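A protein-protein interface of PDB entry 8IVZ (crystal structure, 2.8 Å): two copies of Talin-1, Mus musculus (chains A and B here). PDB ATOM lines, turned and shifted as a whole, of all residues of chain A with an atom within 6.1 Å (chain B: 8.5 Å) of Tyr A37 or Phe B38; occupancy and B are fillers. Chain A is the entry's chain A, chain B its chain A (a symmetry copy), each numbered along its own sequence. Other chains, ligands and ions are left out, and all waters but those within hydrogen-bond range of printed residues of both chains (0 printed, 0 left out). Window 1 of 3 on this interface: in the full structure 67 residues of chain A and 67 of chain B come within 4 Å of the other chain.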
ATOM      1  N   MET A  35      -1.030 -16.057  22.183  1.00  0.00           N
ATOM      2  CA  MET A  35      -1.302 -15.177  21.056  1.00  0.00           C
ATOM      3  C   MET A  35      -0.053 -14.388  20.686  1.00  0.00           C
ATOM      4  O   MET A  35       0.637 -13.852  21.560  1.00  0.00           O
ATOM      5  CB  MET A  35      -2.446 -14.218  21.382  1.00  0.00           C
ATOM      6  CG  MET A  35      -3.829 -14.845  21.336  1.00  0.00           C
ATOM      7  SD  MET A  35      -5.136 -13.602  21.384  1.00  0.00           S
ATOM      8  CE  MET A  35      -4.725 -12.750  22.901  1.00  0.00           C
ATOM      9  N   SER A  36       0.238 -14.321  19.391  1.00  0.00           N
ATOM     10  CA  SER A  36       1.307 -13.464  18.905  1.00  0.00           C
ATOM     11  C   SER A  36       0.852 -12.008  18.944  1.00  0.00           C
ATOM     12  O   SER A  36      -0.279 -11.690  19.325  1.00  0.00           O
ATOM     13  CB  SER A  36       1.716 -13.873  17.492  1.00  0.00           C
ATOM     14  OG  SER A  36       0.656 -13.654  16.577  1.00  0.00           O
ATOM     15  N   TYR A  37       1.747 -11.100  18.547  1.00  0.00           N
ATOM     16  CA  TYR A  37       1.363  -9.695  18.488  1.00  0.00           C
ATOM     17  C   TYR A  37       0.283  -9.461  17.440  1.00  0.00           C
ATOM     18  O   TYR A  37      -0.564  -8.576  17.606  1.00  0.00           O
ATOM     19  CB  TYR A  37       2.583  -8.818  18.208  1.00  0.00           C
ATOM     20  CG  TYR A  37       2.349  -7.352  18.498  1.00  0.00           C
ATOM     21  CD1 TYR A  37       2.534  -6.839  19.777  1.00  0.00           C
ATOM     22  CD2 TYR A  37       1.935  -6.483  17.498  1.00  0.00           C
ATOM     23  CE1 TYR A  37       2.317  -5.500  20.048  1.00  0.00           C
ATOM     24  CE2 TYR A  37       1.715  -5.143  17.760  1.00  0.00           C
ATOM     25  CZ  TYR A  37       1.908  -4.658  19.036  1.00  0.00           C
ATOM     26  OH  TYR A  37       1.690  -3.326  19.299  1.00  0.00           O
ATOM     27  N   PHE A  38       0.292 -10.248  16.362  1.00  0.00           N
ATOM     28  CA  PHE A  38      -0.786 -10.171  15.382  1.00  0.00           C
ATOM     29  C   PHE A  38      -2.052 -10.839  15.900  1.00  0.00           C
ATOM     30  O   PHE A  38      -3.165 -10.390  15.602  1.00  0.00           O
ATOM     31  CB  PHE A  38      -0.348 -10.801  14.062  1.00  0.00           C
ATOM     32  CG  PHE A  38       0.266  -9.825  13.105  1.00  0.00           C
ATOM     33  CD1 PHE A  38       1.549  -9.348  13.311  1.00  0.00           C
ATOM     34  CD2 PHE A  38      -0.441  -9.380  12.002  1.00  0.00           C
ATOM     35  CE1 PHE A  38       2.115  -8.447  12.431  1.00  0.00           C
ATOM     36  CE2 PHE A  38       0.119  -8.481  11.120  1.00  0.00           C
ATOM     37  CZ  PHE A  38       1.398  -8.012  11.336  1.00  0.00           C
ATOM     38  N   GLY A  39      -1.905 -11.918  16.671  1.00  0.00           N
ATOM     39  CA  GLY A  39      -3.065 -12.531  17.292  1.00  0.00           C
ATOM     40  C   GLY A  39      -3.730 -11.625  18.307  1.00  0.00           C
ATOM     41  O   GLY A  39      -4.945 -11.699  18.509  1.00  0.00           O
ATOM     42  N   CYS A  40      -2.951 -10.755  18.953  1.00  0.00           N
ATOM     43  CA  CYS A  40      -3.525  -9.822  19.916  1.00  0.00           C
ATOM     44  C   CYS A  40      -4.333  -8.740  19.213  1.00  0.00           C
ATOM     45  O   CYS A  40      -5.461  -8.435  19.616  1.00  0.00           O
ATOM     46  CB  CYS A  40      -2.422  -9.200  20.771  1.00  0.00           C
ATOM     47  SG  CYS A  40      -1.599 -10.360  21.876  1.00  0.00           S
ATOM     48  N   LEU A  41      -3.772  -8.146  18.156  1.00  0.00           N
ATOM     49  CA  LEU A  41      -4.492  -7.095  17.447  1.00  0.00           C
ATOM     50  C   LEU A  41      -5.737  -7.644  16.764  1.00  0.00           C
ATOM     51  O   LEU A  41      -6.800  -7.016  16.811  1.00  0.00           O
ATOM     52  CB  LEU A  41      -3.579  -6.412  16.430  1.00  0.00           C
ATOM     53  CG  LEU A  41      -4.228  -5.226  15.710  1.00  0.00           C
ATOM     54  CD1 LEU A  41      -4.714  -4.193  16.713  1.00  0.00           C
ATOM     55  CD2 LEU A  41      -3.274  -4.594  14.714  1.00  0.00           C
ATOM     56  N   ASP A  42      -5.630  -8.815  16.130  1.00  0.00           N
ATOM     57  CA  ASP A  42      -6.798  -9.422  15.500  1.00  0.00           C
ATOM     58  C   ASP A  42      -7.899  -9.681  16.520  1.00  0.00           C
ATOM     59  O   ASP A  42      -9.081  -9.453  16.240  1.00  0.00           O
ATOM     60  CB  ASP A  42      -6.406 -10.719  14.792  1.00  0.00           C
ATOM     61  CG  ASP A  42      -5.610 -10.475  13.524  1.00  0.00           C
ATOM     62  OD1 ASP A  42      -5.232  -9.312  13.273  1.00  0.00           O
ATOM     63  OD2 ASP A  42      -5.369 -11.445  12.774  1.00  0.00           O
ATOM     64  N   GLN A  90      -1.761  -9.242  26.905  1.00  0.00           N
ATOM     65  CA  GLN A  90      -0.656  -9.924  26.238  1.00  0.00           C
ATOM     66  C   GLN A  90       0.104  -8.972  25.321  1.00  0.00           C
ATOM     67  O   GLN A  90       1.337  -9.022  25.250  1.00  0.00           O
ATOM     68  CB  GLN A  90      -1.179 -11.131  25.458  1.00  0.00           C
ATOM     69  CG  GLN A  90      -0.120 -11.882  24.658  1.00  0.00           C
ATOM     70  CD  GLN A  90       0.801 -12.723  25.523  1.00  0.00           C
ATOM     71  OE1 GLN A  90       0.609 -12.835  26.734  1.00  0.00           O
ATOM     72  NE2 GLN A  90       1.807 -13.324  24.900  1.00  0.00           N
ATOM     73  N   ALA A  91      -0.615  -8.093  24.616  1.00  0.00           N
ATOM     74  CA  ALA A  91       0.051  -7.129  23.746  1.00  0.00           C
ATOM     75  C   ALA A  91       0.906  -6.159  24.551  1.00  0.00           C
ATOM     76  O   ALA A  91       1.989  -5.765  24.105  1.00  0.00           O
ATOM     77  CB  ALA A  91      -0.980  -6.372  22.908  1.00  0.00           C
ATOM     78  N   ALA A  92       0.439  -5.764  25.738  1.00  0.00           N
ATOM     79  CA  ALA A  92       1.248  -4.901  26.591  1.00  0.00           C
ATOM     80  C   ALA A  92       2.507  -5.620  27.058  1.00  0.00           C
ATOM     81  O   ALA A  92       3.578  -5.010  27.157  1.00  0.00           O
ATOM     82  CB  ALA A  92       0.426  -4.419  27.785  1.00  0.00           C
ATOM     83  N   LEU A  94       4.063  -8.000  25.332  1.00  0.00           N
ATOM     84  CA  LEU A  94       4.956  -8.127  24.185  1.00  0.00           C
ATOM     85  C   LEU A  94       5.620  -6.801  23.836  1.00  0.00           C
ATOM     86  O   LEU A  94       6.755  -6.791  23.345  1.00  0.00           O
ATOM     87  CB  LEU A  94       4.191  -8.673  22.979  1.00  0.00           C
ATOM     88  CG  LEU A  94       3.586 -10.072  23.118  1.00  0.00           C
ATOM     89  CD1 LEU A  94       2.836 -10.460  21.854  1.00  0.00           C
ATOM     90  CD2 LEU A  94       4.657 -11.101  23.446  1.00  0.00           C
ATOM     91  N   VAL A  95       4.942  -5.680  24.080  1.00  0.00           N
ATOM     92  CA  VAL A  95       5.508  -4.379  23.730  1.00  0.00           C
ATOM     93  C   VAL A  95       6.738  -4.084  24.580  1.00  0.00           C
ATOM     94  O   VAL A  95       7.810  -3.759  24.057  1.00  0.00           O
ATOM     95  CB  VAL A  95       4.443  -3.274  23.865  1.00  0.00           C
ATOM     96  CG1 VAL A  95       5.100  -1.907  23.938  1.00  0.00           C
ATOM     97  CG2 VAL A  95       3.476  -3.329  22.693  1.00  0.00           C
ATOM     98  N   SER A  98       9.581  -6.511  23.754  1.00  0.00           N
ATOM     99  CA  SER A  98      10.187  -6.256  22.453  1.00  0.00           C
ATOM    100  C   SER A  98      10.956  -4.939  22.396  1.00  0.00           C
ATOM    101  O   SER A  98      11.373  -4.534  21.306  1.00  0.00           O
ATOM    102  CB  SER A  98       9.119  -6.268  21.357  1.00  0.00           C
ATOM    103  OG  SER A  98       8.181  -5.223  21.547  1.00  0.00           O
ATOM    104  N   MET B  35      12.725  -1.104  14.996  1.00  0.00           N
ATOM    105  CA  MET B  35      11.476  -1.448  14.331  1.00  0.00           C
ATOM    106  C   MET B  35      10.653  -2.386  15.202  1.00  0.00           C
ATOM    107  O   MET B  35      11.179  -3.352  15.764  1.00  0.00           O
ATOM    108  CB  MET B  35      11.747  -2.098  12.975  1.00  0.00           C
ATOM    109  CG  MET B  35      12.164  -1.130  11.881  1.00  0.00           C
ATOM    110  SD  MET B  35      12.128  -1.898  10.249  1.00  0.00           S
ATOM    111  CE  MET B  35      13.227  -3.284  10.512  1.00  0.00           C
ATOM    112  N   SER B  36       9.359  -2.100  15.315  1.00  0.00           N
ATOM    113  CA  SER B  36       8.444  -3.011  15.982  1.00  0.00           C
ATOM    114  C   SER B  36       8.166  -4.208  15.077  1.00  0.00           C
ATOM    115  O   SER B  36       8.665  -4.302  13.952  1.00  0.00           O
ATOM    116  CB  SER B  36       7.150  -2.289  16.352  1.00  0.00           C
ATOM    117  OG  SER B  36       6.448  -1.886  15.189  1.00  0.00           O
ATOM    118  N   TYR B  37       7.355  -5.145  15.574  1.00  0.00           N
ATOM    119  CA  TYR B  37       6.983  -6.284  14.743  1.00  0.00           C
ATOM    120  C   TYR B  37       6.157  -5.845  13.542  1.00  0.00           C
ATOM    121  O   TYR B  37       6.237  -6.459  12.472  1.00  0.00           O
ATOM    122  CB  TYR B  37       6.225  -7.324  15.567  1.00  0.00           C
ATOM    123  CG  TYR B  37       6.134  -8.675  14.893  1.00  0.00           C
ATOM    124  CD1 TYR B  37       7.150  -9.612  15.032  1.00  0.00           C
ATOM    125  CD2 TYR B  37       5.037  -9.010  14.111  1.00  0.00           C
ATOM    126  CE1 TYR B  37       7.074 -10.847  14.414  1.00  0.00           C
ATOM    127  CE2 TYR B  37       4.952 -10.242  13.489  1.00  0.00           C
ATOM    128  CZ  TYR B  37       5.972 -11.156  13.644  1.00  0.00           C
ATOM    129  OH  TYR B  37       5.889 -12.382  13.026  1.00  0.00           O
ATOM    130  N   PHE B  38       5.365  -4.782  13.697  1.00  0.00           N
ATOM    131  CA  PHE B  38       4.645  -4.224  12.556  1.00  0.00           C
ATOM    132  C   PHE B  38       5.578  -3.438  11.646  1.00  0.00           C
ATOM    133  O   PHE B  38       5.400  -3.432  10.422  1.00  0.00           O
ATOM    134  CB  PHE B  38       3.494  -3.342  13.036  1.00  0.00           C
ATOM    135  CG  PHE B  38       2.198  -4.077  13.188  1.00  0.00           C
ATOM    136  CD1 PHE B  38       1.994  -4.935  14.255  1.00  0.00           C
ATOM    137  CD2 PHE B  38       1.184  -3.914  12.261  1.00  0.00           C
ATOM    138  CE1 PHE B  38       0.800  -5.615  14.394  1.00  0.00           C
ATOM    139  CE2 PHE B  38      -0.011  -4.589  12.396  1.00  0.00           C
ATOM    140  CZ  PHE B  38      -0.202  -5.442  13.463  1.00  0.00           C
ATOM    141  N   GLY B  39       6.573  -2.762  12.222  1.00  0.00           N
ATOM    142  CA  GLY B  39       7.566  -2.090  11.403  1.00  0.00           C
ATOM    143  C   GLY B  39       8.399  -3.055  10.587  1.00  0.00           C
ATOM    144  O   GLY B  39       8.859  -2.715   9.494  1.00  0.00           O
ATOM    145  N   CYS B  40       8.602  -4.272  11.098  1.00  0.00           N
ATOM    146  CA  CYS B  40       9.360  -5.270  10.352  1.00  0.00           C
ATOM    147  C   CYS B  40       8.562  -5.785   9.163  1.00  0.00           C
ATOM    148  O   CYS B  40       9.086  -5.877   8.047  1.00  0.00           O
ATOM    149  CB  CYS B  40       9.761  -6.423  11.272  1.00  0.00           C
ATOM    150  SG  CYS B  40      10.954  -5.975  12.544  1.00  0.00           S
ATOM    151  N   LEU B  41       7.290  -6.128   9.380  1.00  0.00           N
ATOM    152  CA  LEU B  41       6.478  -6.639   8.282  1.00  0.00           C
ATOM    153  C   LEU B  41       6.246  -5.568   7.224  1.00  0.00           C
ATOM    154  O   LEU B  41       6.332  -5.851   6.024  1.00  0.00           O
ATOM    155  CB  LEU B  41       5.145  -7.173   8.805  1.00  0.00           C
ATOM    156  CG  LEU B  41       4.270  -7.820   7.727  1.00  0.00           C
ATOM    157  CD1 LEU B  41       5.021  -8.947   7.035  1.00  0.00           C
ATOM    158  CD2 LEU B  41       2.964  -8.328   8.307  1.00  0.00           C
ATOM    159  N   ASP B  42       5.959  -4.333   7.645  1.00  0.00           N
ATOM    160  CA  ASP B  42       5.778  -3.250   6.684  1.00  0.00           C
ATOM    161  C   ASP B  42       7.033  -3.045   5.845  1.00  0.00           C
ATOM    162  O   ASP B  42       6.948  -2.826   4.632  1.00  0.00           O
ATOM    163  CB  ASP B  42       5.397  -1.956   7.406  1.00  0.00           C
ATOM    164  CG  ASP B  42       3.977  -1.980   7.938  1.00  0.00           C
ATOM    165  OD1 ASP B  42       3.337  -3.052   7.881  1.00  0.00           O
ATOM    166  OD2 ASP B  42       3.496  -0.926   8.405  1.00  0.00           O
ATOM    167  N   SER B  43       8.208  -3.115   6.476  1.00  0.00           N
ATOM    168  CA  SER B  43       9.453  -3.010   5.724  1.00  0.00           C
ATOM    169  C   SER B  43       9.611  -4.162   4.743  1.00  0.00           C
ATOM    170  O   SER B  43      10.181  -3.984   3.661  1.00  0.00           O
ATOM    171  CB  SER B  43      10.645  -2.960   6.681  1.00  0.00           C
ATOM    172  OG  SER B  43      11.871  -2.951   5.971  1.00  0.00           O
ATOM    173  N   VAL B  44       9.115  -5.349   5.101  1.00  0.00           N
ATOM    174  CA  VAL B  44       9.172  -6.483   4.187  1.00  0.00           C
ATOM    175  C   VAL B  44       8.238  -6.260   3.004  1.00  0.00           C
ATOM    176  O   VAL B  44       8.595  -6.541   1.854  1.00  0.00           O
ATOM    177  CB  VAL B  44       8.846  -7.787   4.939  1.00  0.00           C
ATOM    178  CG1 VAL B  44       8.628  -8.931   3.963  1.00  0.00           C
ATOM    179  CG2 VAL B  44       9.963  -8.128   5.912  1.00  0.00           C
ATOM    180  N   MET B  45       7.036  -5.736   3.262  1.00  0.00           N
ATOM    181  CA  MET B  45       6.079  -5.511   2.182  1.00  0.00           C
ATOM    182  C   MET B  45       6.574  -4.444   1.214  1.00  0.00           C
ATOM    183  O   MET B  45       6.477  -4.615  -0.006  1.00  0.00           O
ATOM    184  CB  MET B  45       4.718  -5.118   2.760  1.00  0.00           C
ATOM    185  CG  MET B  45       4.172  -6.091   3.794  1.00  0.00           C
ATOM    186  SD  MET B  45       3.599  -7.652   3.100  1.00  0.00           S
ATOM    187  CE  MET B  45       1.995  -7.168   2.471  1.00  0.00           C
ATOM    188  N   ALA B  87      14.775  -6.240   8.305  1.00  0.00           N
ATOM    189  CA  ALA B  87      13.461  -6.478   8.887  1.00  0.00           C
ATOM    190  C   ALA B  87      13.305  -7.931   9.312  1.00  0.00           C
ATOM    191  O   ALA B  87      12.773  -8.213  10.391  1.00  0.00           O
ATOM    192  CB  ALA B  87      12.369  -6.081   7.894  1.00  0.00           C
ATOM    193  N   GLN B  90      15.389  -8.601  12.554  1.00  0.00           N
ATOM    194  CA  GLN B  90      14.729  -8.077  13.745  1.00  0.00           C
ATOM    195  C   GLN B  90      13.446  -8.844  14.046  1.00  0.00           C
ATOM    196  O   GLN B  90      13.141  -9.121  15.211  1.00  0.00           O
ATOM    197  CB  GLN B  90      14.443  -6.585  13.572  1.00  0.00           C
ATOM    198  CG  GLN B  90      13.687  -5.940  14.729  1.00  0.00           C
ATOM    199  CD  GLN B  90      14.546  -5.727  15.962  1.00  0.00           C
ATOM    200  OE1 GLN B  90      15.751  -5.973  15.948  1.00  0.00           O
ATOM    201  NE2 GLN B  90      13.924  -5.262  17.039  1.00  0.00           N
ATOM    202  N   ALA B  91      12.685  -9.201  13.006  1.00  0.00           N
ATOM    203  CA  ALA B  91      11.462  -9.967  13.219  1.00  0.00           C
ATOM    204  C   ALA B  91      11.770 -11.348  13.785  1.00  0.00           C
ATOM    205  O   ALA B  91      11.019 -11.860  14.623  1.00  0.00           O
ATOM    206  CB  ALA B  91      10.675 -10.083  11.914  1.00  0.00           C
ATOM    207  N   LEU B  94      12.372 -10.834  17.437  1.00  0.00           N
ATOM    208  CA  LEU B  94      11.149 -10.591  18.196  1.00  0.00           C
ATOM    209  C   LEU B  94      10.314 -11.856  18.343  1.00  0.00           C
ATOM    210  O   LEU B  94       9.618 -12.021  19.351  1.00  0.00           O
ATOM    211  CB  LEU B  94      10.329  -9.485  17.531  1.00  0.00           C
ATOM    212  CG  LEU B  94      10.976  -8.102  17.442  1.00  0.00           C
ATOM    213  CD1 LEU B  94      10.053  -7.122  16.733  1.00  0.00           C
ATOM    214  CD2 LEU B  94      11.352  -7.584  18.822  1.00  0.00           C
ATOM    215  N   VAL B  95      10.367 -12.757  17.361  1.00  0.00           N
ATOM    216  CA  VAL B  95       9.558 -13.972  17.424  1.00  0.00           C
ATOM    217  C   VAL B  95      10.020 -14.865  18.570  1.00  0.00           C
ATOM    218  O   VAL B  95       9.219 -15.286  19.412  1.00  0.00           O
ATOM    219  CB  VAL B  95       9.592 -14.713  16.074  1.00  0.00           C
ATOM    220  CG1 VAL B  95       9.141 -16.154  16.245  1.00  0.00           C
ATOM    221  CG2 VAL B  95       8.707 -14.004  15.062  1.00  0.00           C
ATOM    222  N   SER B  98       9.344 -13.203  21.952  1.00  0.00           N
ATOM    223  CA  SER B  98       7.928 -13.172  22.298  1.00  0.00           C
ATOM    224  C   SER B  98       7.348 -14.555  22.577  1.00  0.00           C
ATOM    225  O   SER B  98       6.126 -14.676  22.718  1.00  0.00           O
ATOM    226  CB  SER B  98       7.123 -12.498  21.184  1.00  0.00           C
ATOM    227  OG  SER B  98       7.199 -13.239  19.979  1.00  0.00           O
ATOM    228  N   ALA B 113       6.527   2.189  27.286  1.00  0.00           N
ATOM    229  CA  ALA B 113       5.861   1.979  26.008  1.00  0.00           C
ATOM    230  C   ALA B 113       4.599   1.139  26.130  1.00  0.00           C
ATOM    231  O   ALA B 113       3.672   1.311  25.329  1.00  0.00           O
ATOM    232  CB  ALA B 113       6.822   1.319  25.014  1.00  0.00           C
ATOM    233  N   ILE B 117      -0.903   1.314  26.514  1.00  0.00           N
ATOM    234  CA  ILE B 117      -1.809   0.202  26.254  1.00  0.00           C
ATOM    235  C   ILE B 117      -2.543  -0.202  27.527  1.00  0.00           C
ATOM    236  O   ILE B 117      -3.741  -0.509  27.497  1.00  0.00           O
ATOM    237  CB  ILE B 117      -1.023  -0.974  25.645  1.00  0.00           C
ATOM    238  CG1 ILE B 117      -0.572  -0.626  24.223  1.00  0.00           C
ATOM    239  CG2 ILE B 117      -1.843  -2.258  25.664  1.00  0.00           C
ATOM    240  CD1 ILE B 117       0.268  -1.697  23.568  1.00  0.00           C
ATOM    241  N   LEU B 165      -6.435   2.638  22.219  1.00  0.00           N
ATOM    242  CA  LEU B 165      -5.745   1.372  22.435  1.00  0.00           C
ATOM    243  C   LEU B 165      -5.236   0.791  21.122  1.00  0.00           C
ATOM    244  O   LEU B 165      -4.090   0.337  21.039  1.00  0.00           O
ATOM    245  CB  LEU B 165      -6.672   0.377  23.137  1.00  0.00           C
ATOM    246  CG  LEU B 165      -6.076  -1.010  23.388  1.00  0.00           C
ATOM    247  CD1 LEU B 165      -4.772  -0.888  24.152  1.00  0.00           C
ATOM    248  CD2 LEU B 165      -7.052  -1.891  24.143  1.00  0.00           C
ATOM    249  N   ILE B 166      -6.078   0.792  20.086  1.00  0.00           N
ATOM    250  CA  ILE B 166      -5.651   0.295  18.782  1.00  0.00           C
ATOM    251  C   ILE B 166      -4.542   1.171  18.219  1.00  0.00           C
ATOM    252  O   ILE B 166      -3.562   0.673  17.652  1.00  0.00           O
ATOM    253  CB  ILE B 166      -6.852   0.213  17.821  1.00  0.00           C
ATOM    254  CG1 ILE B 166      -7.960  -0.653  18.426  1.00  0.00           C
ATOM    255  CG2 ILE B 166      -6.422  -0.341  16.472  1.00  0.00           C
ATOM    256  CD1 ILE B 166      -9.224  -0.694  17.599  1.00  0.00           C
ATOM    257  N   THR B 167      -4.672   2.491  18.377  1.00  0.00           N
ATOM    258  CA  THR B 167      -3.635   3.403  17.906  1.00  0.00           C
ATOM    259  C   THR B 167      -2.309   3.154  18.615  1.00  0.00           C
ATOM    260  O   THR B 167      -1.243   3.317  18.011  1.00  0.00           O
ATOM    261  CB  THR B 167      -4.085   4.852  18.105  1.00  0.00           C
ATOM    262  OG1 THR B 167      -5.405   5.020  17.572  1.00  0.00           O
ATOM    263  CG2 THR B 167      -3.140   5.810  17.395  1.00  0.00           C
ATOM    264  N   SER B 168      -2.353   2.748  19.886  1.00  0.00           N
ATOM    265  CA  SER B 168      -1.127   2.475  20.626  1.00  0.00           C
ATOM    266  C   SER B 168      -0.432   1.205  20.152  1.00  0.00           C
ATOM    267  O   SER B 168       0.775   1.056  20.371  1.00  0.00           O
ATOM    268  CB  SER B 168      -1.428   2.378  22.123  1.00  0.00           C
ATOM    269  OG  SER B 168      -2.031   3.567  22.603  1.00  0.00           O
ATOM    270  N   MET B 169      -1.158   0.293  19.503  1.00  0.00           N
ATOM    271  CA  MET B 169      -0.596  -0.976  19.060  1.00  0.00           C
ATOM    272  C   MET B 169      -0.139  -0.966  17.608  1.00  0.00           C
ATOM    273  O   MET B 169       0.755  -1.739  17.248  1.00  0.00           O
ATOM    274  CB  MET B 169      -1.617  -2.104  19.248  1.00  0.00           C
ATOM    275  CG  MET B 169      -1.941  -2.427  20.699  1.00  0.00           C
ATOM    276  SD  MET B 169      -3.133  -3.770  20.873  1.00  0.00           S
ATOM    277  CE  MET B 169      -4.622  -2.994  20.253  1.00  0.00           C
ATOM    278  N   ARG B 170      -0.723  -0.112  16.764  1.00  0.00           N
ATOM    279  CA  ARG B 170      -0.428  -0.150  15.338  1.00  0.00           C
ATOM    280  C   ARG B 170       0.925   0.454  14.989  1.00  0.00           C
ATOM    281  O   ARG B 170       1.484   0.114  13.940  1.00  0.00           O
ATOM    282  CB  ARG B 170      -1.526   0.570  14.555  1.00  0.00           C
ATOM    283  CG  ARG B 170      -2.883  -0.098  14.646  1.00  0.00           C
ATOM    284  CD  ARG B 170      -3.862   0.514  13.664  1.00  0.00           C
ATOM    285  NE  ARG B 170      -3.326   0.541  12.307  1.00  0.00           N
ATOM    286  CZ  ARG B 170      -3.267  -0.517  11.503  1.00  0.00           C
ATOM    287  NH1 ARG B 170      -2.762  -0.395  10.283  1.00  0.00           N
ATOM    288  NH2 ARG B 170      -3.707  -1.697  11.920  1.00  0.00           N
ATOM    289  N   ASP B 171       1.462   1.333  15.827  1.00  0.00           N
ATOM    290  CA  ASP B 171       2.751   1.952  15.542  1.00  0.00           C
ATOM    291  C   ASP B 171       3.896   1.017  15.918  1.00  0.00           C
ATOM    292  O   ASP B 171       4.455   0.329  15.064  1.00  0.00           O
ATOM    293  CB  ASP B 171       2.889   3.281  16.286  1.00  0.00           C
ATOM    294  CG  ASP B 171       4.073   4.097  15.805  1.00  0.00           C
ATOM    295  OD1 ASP B 171       4.585   3.813  14.701  1.00  0.00           O
ATOM    296  OD2 ASP B 171       4.497   5.019  16.534  1.00  0.00           O
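The backbone carbonyl oxygen of Met B169 lies within hydrogen-bond range of the side-chain hydroxyl of Tyr A37, at 2.8 Å.
Tyr A37 touches two residues of chain B.
Of chain B, only Tyr B37 (3.4 Å), Phe B38 (3.7 Å) and Leu B41 (3.4 Å) come within 4 Å of Phe A38.
Printed residues of chain B within 4 Å of Ser A98: Leu B94 (3.6 Å).
Phe B38 touches just these residues of chain A: Tyr A37, Phe A38 and Leu A41.
Of the printed residues of chain A, Leu B41 touches Phe A38.
Ser B43 touches none of the printed residues of chain A.
The nearest residue of chain B that does not touch Tyr A37 is Ser B168 (4.6 Å).
The nearest printed residue of chain A that does not touch Phe B38 is Asp A42 (6.3 Å).
The backbone carbonyl oxygen (O) of Leu B94 lies within hydrogen-bond range of the side-chain hydroxyl (OG) of Ser B98 (2.8 Å).
The backbone NH of Ala A91 is in hydrogen-bond range of the side-chain sulfur of Cys A40.
The backbone NH (N) of Phe A38 sits close to the side-chain hydroxyl (OG) of Ser A36 (3.4 Å).
OG of Ser A98 lies within hydrogen-bond range of O of Leu A94 (2.8 Å).
N of Phe B38 sits close to OG of Ser B36 (3.4 Å).
O of Val A95 sits at hydrogen-bond distance from OG of Ser A98 (2.9 Å).
Among the printed residues, merely in contact across the chains: Tyr A37 with Phe B38 (3.4 Å), Phe A38 with Tyr B37 (3.4 Å), Phe A38 with Phe B38 (3.7 Å), Phe A38 with Leu B41 (3.4 Å), Leu A41 with Phe B38 (3.4 Å), Leu A41 with Met B169 (3.7 Å), Ala A91 with Met B169 (3.9 Å), Ala A92 with Ile B117 (3.8 Å), Leu A94 with Ser B98 (3.6 Å), Val A95 with Ala B113 (3.8 Å), Val A95 with Ile B117 (3.7 Å) and Ser A98 with Leu B94 (3.6 Å).
Tyr A37 touches Phe B38, and with the chains exchanged Phe A38 touches Tyr B37.
Phe B38 touches its own counterpart, Phe A38.
Phe A38 touches Leu B41, and with the chains exchanged Leu A41 touches Phe B38.
Leu A94 touches Ser B98, and with the chains exchanged Ser A98 touches Leu B94.
13 positions are printed for both chains.
Printed residues of chain A that touch a printed residue of chain B: Tyr A37, Phe A38, Leu A41, Ala A91, Ala A92, Leu A94, Val A95 and Ser A98.
Of the 26 printed residues of chain B, 8 touch a printed residue of chain A.
Hydrophobic or aromatic side chains of chain B within 4 Å of the printed part of chain A: Tyr B37, Phe B38, Leu B41, Leu B94, Ala B113, Ile B117 and Met B169.
Among the printed residues, 13 pairs touch across the chains.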
